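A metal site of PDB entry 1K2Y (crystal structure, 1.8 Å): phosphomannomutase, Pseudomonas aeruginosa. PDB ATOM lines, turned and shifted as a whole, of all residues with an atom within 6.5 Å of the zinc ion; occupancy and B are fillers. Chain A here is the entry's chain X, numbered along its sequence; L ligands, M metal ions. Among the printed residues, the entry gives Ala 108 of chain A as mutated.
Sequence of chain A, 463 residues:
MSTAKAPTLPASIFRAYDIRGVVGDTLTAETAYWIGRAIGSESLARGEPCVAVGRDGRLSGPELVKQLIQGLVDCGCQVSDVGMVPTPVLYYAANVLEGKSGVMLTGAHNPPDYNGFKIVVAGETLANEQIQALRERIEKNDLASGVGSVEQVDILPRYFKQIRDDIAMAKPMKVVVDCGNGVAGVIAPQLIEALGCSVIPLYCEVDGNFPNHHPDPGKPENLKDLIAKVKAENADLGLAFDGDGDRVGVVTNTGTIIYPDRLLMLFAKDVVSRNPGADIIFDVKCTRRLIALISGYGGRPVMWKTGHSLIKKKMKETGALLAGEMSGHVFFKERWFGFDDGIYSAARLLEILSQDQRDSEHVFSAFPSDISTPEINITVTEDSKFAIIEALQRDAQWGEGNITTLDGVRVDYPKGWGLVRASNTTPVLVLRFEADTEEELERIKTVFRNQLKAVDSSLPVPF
The side-chain carboxylate (OD2) of Asp 246 is in salt-bridge range of the side-chain amino group (NZ) of Lys 118, 2.9 Å away. The backbone NH (N) of Asp 242 is in hydrogen-bond range of the backbone carbonyl oxygen (O) of Arg 247, at 3.1 Å. OD1 of Asp 242 lies within hydrogen-bond range of N of Gly 245 (2.9 Å). OD1 of Asp 244 lies within salt-bridge range of NZ of Lys 118 (2.8 Å). The side-chain carboxylate (OD1) of Asp 244 is in hydrogen-bond range of the side-chain hydroxyl (OG1) of Thr 87 (2.7 Å).
Lys 118 touches the zinc ion. Four residues have an atom within 4 Å of the zinc ion: Lys 118, Asp 242, Asp 244 and Asp 246. The nearest printed residue that does not touch the zinc ion is Ala 108 (4.1 Å).
An oxygen (O1) of the ligand is bound to the zinc ion, at 1.9 Å. OD1 of Asp 246 binds the zinc ion (1.9 Å). OD2 of Asp 242 binds the zinc ion. OD2 of Asp 244 binds the zinc ion (2.0 Å). The zinc ion has four donor atoms within binding distance.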
ATOM      1  N   THR A  87     -31.057  22.041  -5.824  1.00  0.00           N
ATOM      2  CA  THR A  87     -31.549  23.411  -5.904  1.00  0.00           C
ATOM      3  C   THR A  87     -32.088  23.800  -7.276  1.00  0.00           C
ATOM      4  O   THR A  87     -33.181  24.377  -7.367  1.00  0.00           O
ATOM      5  CB  THR A  87     -30.438  24.366  -5.498  1.00  0.00           C
ATOM      6  OG1 THR A  87     -30.278  24.294  -4.069  1.00  0.00           O
ATOM      7  CG2 THR A  87     -30.789  25.804  -5.831  1.00  0.00           C
ATOM      8  N   THR A 106     -31.816  24.550   1.968  1.00  0.00           N
ATOM      9  CA  THR A 106     -30.507  23.983   1.744  1.00  0.00           C
ATOM     10  C   THR A 106     -29.398  24.766   2.471  1.00  0.00           C
ATOM     11  O   THR A 106     -29.513  25.955   2.667  1.00  0.00           O
ATOM     12  CB  THR A 106     -30.183  23.944   0.189  1.00  0.00           C
ATOM     13  OG1 THR A 106     -28.860  23.422  -0.013  1.00  0.00           O
ATOM     14  CG2 THR A 106     -30.145  25.345  -0.424  1.00  0.00           C
ATOM     15  N   ALA A 108     -26.401  24.249   1.132  1.00  0.00           N
ATOM     16  CA  ALA A 108     -25.534  24.340  -0.038  1.00  0.00           C
ATOM     17  C   ALA A 108     -24.278  23.509   0.094  1.00  0.00           C
ATOM     18  O   ALA A 108     -24.342  22.281   0.183  1.00  0.00           O
ATOM     19  CB  ALA A 108     -25.206  25.832  -0.324  1.00  0.00           C
ATOM     20  N   HIS A 109     -23.112  24.167   0.132  1.00  0.00           N
ATOM     21  CA  HIS A 109     -21.826  23.496   0.162  1.00  0.00           C
ATOM     22  C   HIS A 109     -21.200  23.515   1.566  1.00  0.00           C
ATOM     23  O   HIS A 109     -20.086  23.037   1.755  1.00  0.00           O
ATOM     24  CB  HIS A 109     -20.838  24.261  -0.742  1.00  0.00           C
ATOM     25  CG  HIS A 109     -20.637  25.670  -0.313  1.00  0.00           C
ATOM     26  ND1 HIS A 109     -21.660  26.583  -0.251  1.00  0.00           N
ATOM     27  CD2 HIS A 109     -19.518  26.327   0.080  1.00  0.00           C
ATOM     28  CE1 HIS A 109     -21.186  27.744   0.167  1.00  0.00           C
ATOM     29  NE2 HIS A 109     -19.886  27.621   0.355  1.00  0.00           N
ATOM     30  N   LYS A 118     -33.230  29.382   0.161  1.00  0.00           N
ATOM     31  CA  LYS A 118     -33.078  30.109  -1.091  1.00  0.00           C
ATOM     32  C   LYS A 118     -34.485  30.355  -1.579  1.00  0.00           C
ATOM     33  O   LYS A 118     -35.289  29.447  -1.716  1.00  0.00           O
ATOM     34  CB  LYS A 118     -32.229  29.333  -2.104  1.00  0.00           C
ATOM     35  CG  LYS A 118     -30.752  29.175  -1.644  1.00  0.00           C
ATOM     36  CD  LYS A 118     -29.865  28.506  -2.703  1.00  0.00           C
ATOM     37  CE  LYS A 118     -28.443  28.371  -2.216  1.00  0.00           C
ATOM     38  NZ  LYS A 118     -27.469  27.806  -3.189  1.00  0.00           N
ATOM     39  N   ASP A 242     -21.352  20.736  -6.318  1.00  0.00           N
ATOM     40  CA  ASP A 242     -21.464  21.238  -4.961  1.00  0.00           C
ATOM     41  C   ASP A 242     -22.677  20.562  -4.288  1.00  0.00           C
ATOM     42  O   ASP A 242     -23.434  19.814  -4.928  1.00  0.00           O
ATOM     43  CB  ASP A 242     -21.418  22.755  -4.878  1.00  0.00           C
ATOM     44  CG  ASP A 242     -22.750  23.411  -5.033  1.00  0.00           C
ATOM     45  OD1 ASP A 242     -23.625  22.881  -5.762  1.00  0.00           O
ATOM     46  OD2 ASP A 242     -22.987  24.525  -4.451  1.00  0.00           O
ATOM     47  N   GLY A 243     -22.855  20.827  -3.007  1.00  0.00           N
ATOM     48  CA  GLY A 243     -23.832  20.077  -2.229  1.00  0.00           C
ATOM     49  C   GLY A 243     -25.260  20.151  -2.673  1.00  0.00           C
ATOM     50  O   GLY A 243     -25.970  19.153  -2.563  1.00  0.00           O
ATOM     51  N   ASP A 244     -25.689  21.298  -3.180  1.00  0.00           N
ATOM     52  CA  ASP A 244     -27.048  21.450  -3.672  1.00  0.00           C
ATOM     53  C   ASP A 244     -27.169  21.400  -5.200  1.00  0.00           C
ATOM     54  O   ASP A 244     -28.299  21.424  -5.740  1.00  0.00           O
ATOM     55  CB  ASP A 244     -27.738  22.660  -3.093  1.00  0.00           C
ATOM     56  CG  ASP A 244     -27.045  23.989  -3.453  1.00  0.00           C
ATOM     57  OD1 ASP A 244     -27.720  25.022  -3.516  1.00  0.00           O
ATOM     58  OD2 ASP A 244     -25.823  24.017  -3.586  1.00  0.00           O
ATOM     59  N   GLY A 245     -26.045  21.317  -5.906  1.00  0.00           N
ATOM     60  CA  GLY A 245     -26.096  21.108  -7.340  1.00  0.00           C
ATOM     61  C   GLY A 245     -26.239  22.337  -8.252  1.00  0.00           C
ATOM     62  O   GLY A 245     -26.507  22.194  -9.476  1.00  0.00           O
ATOM     63  N   ASP A 246     -26.069  23.515  -7.685  1.00  0.00           N
ATOM     64  CA  ASP A 246     -26.090  24.709  -8.538  1.00  0.00           C
ATOM     65  C   ASP A 246     -24.721  25.122  -9.058  1.00  0.00           C
ATOM     66  O   ASP A 246     -24.639  26.162  -9.715  1.00  0.00           O
ATOM     67  CB  ASP A 246     -26.797  25.892  -7.911  1.00  0.00           C
ATOM     68  CG  ASP A 246     -26.213  26.318  -6.590  1.00  0.00           C
ATOM     69  OD1 ASP A 246     -25.204  25.706  -6.134  1.00  0.00           O
ATOM     70  OD2 ASP A 246     -26.803  27.159  -5.908  1.00  0.00           O
ATOM     71  N   ARG A 247     -23.696  24.364  -8.747  1.00  0.00           N
ATOM     72  CA  ARG A 247     -22.333  24.584  -9.256  1.00  0.00           C
ATOM     73  C   ARG A 247     -21.695  23.272  -9.592  1.00  0.00           C
ATOM     74  O   ARG A 247     -21.983  22.262  -8.921  1.00  0.00           O
ATOM     75  CB  ARG A 247     -21.451  25.282  -8.178  1.00  0.00           C
ATOM     76  CG  ARG A 247     -21.899  26.644  -7.765  1.00  0.00           C
ATOM     77  CD  ARG A 247     -20.910  27.336  -6.870  1.00  0.00           C
ATOM     78  NE  ARG A 247     -20.904  26.856  -5.500  1.00  0.00           N
ATOM     79  CZ  ARG A 247     -19.863  26.365  -4.815  1.00  0.00           C
ATOM     80  NH1 ARG A 247     -18.649  26.273  -5.337  1.00  0.00           N
ATOM     81  NH2 ARG A 247     -20.032  26.019  -3.560  1.00  0.00           N
ATOM     82  N   HIS A 329     -21.179  29.784 -10.513  1.00  0.00           N
ATOM     83  CA  HIS A 329     -22.557  29.741 -11.021  1.00  0.00           C
ATOM     84  C   HIS A 329     -22.561  30.103 -12.517  1.00  0.00           C
ATOM     85  O   HIS A 329     -21.962  31.131 -12.941  1.00  0.00           O
ATOM     86  CB  HIS A 329     -23.420  30.736 -10.239  1.00  0.00           C
ATOM     87  CG  HIS A 329     -23.654  30.339  -8.820  1.00  0.00           C
ATOM     88  ND1 HIS A 329     -22.777  30.614  -7.784  1.00  0.00           N
ATOM     89  CD2 HIS A 329     -24.686  29.665  -8.260  1.00  0.00           C
ATOM     90  CE1 HIS A 329     -23.248  30.093  -6.660  1.00  0.00           C
ATOM     91  NE2 HIS A 329     -24.397  29.523  -6.914  1.00  0.00           N
HETATM   92  O1  LIG L   1     -24.715  27.005  -3.334  1.00  0.00           O
HETATM   93  O2  LIG L   1     -22.647  27.664  -3.484  1.00  0.00           O
HETATM   94  C1  LIG L   1     -23.819  27.792  -2.994  1.00  0.00           C
HETATM   95  C2  LIG L   1     -24.108  28.965  -2.092  1.00  0.00           C
HETATM   96  O3  LIG L   1     -25.480  29.069  -1.668  1.00  0.00           O
HETATM   97  C3  LIG L   1     -23.733  30.251  -2.839  1.00  0.00           C
HETATM   98  O4  LIG L   1     -24.467  30.437  -4.053  1.00  0.00           O
HETATM   99  C4  LIG L   1     -23.996  31.477  -2.002  1.00  0.00           C
HETATM  100  O5  LIG L   1     -24.845  32.315  -2.366  1.00  0.00           O
HETATM  101  O6  LIG L   1     -23.397  31.566  -0.949  1.00  0.00           O
HETATM  102 ZN    ZN M   1     -24.624  25.458  -4.358  1.00  0.00          ZN
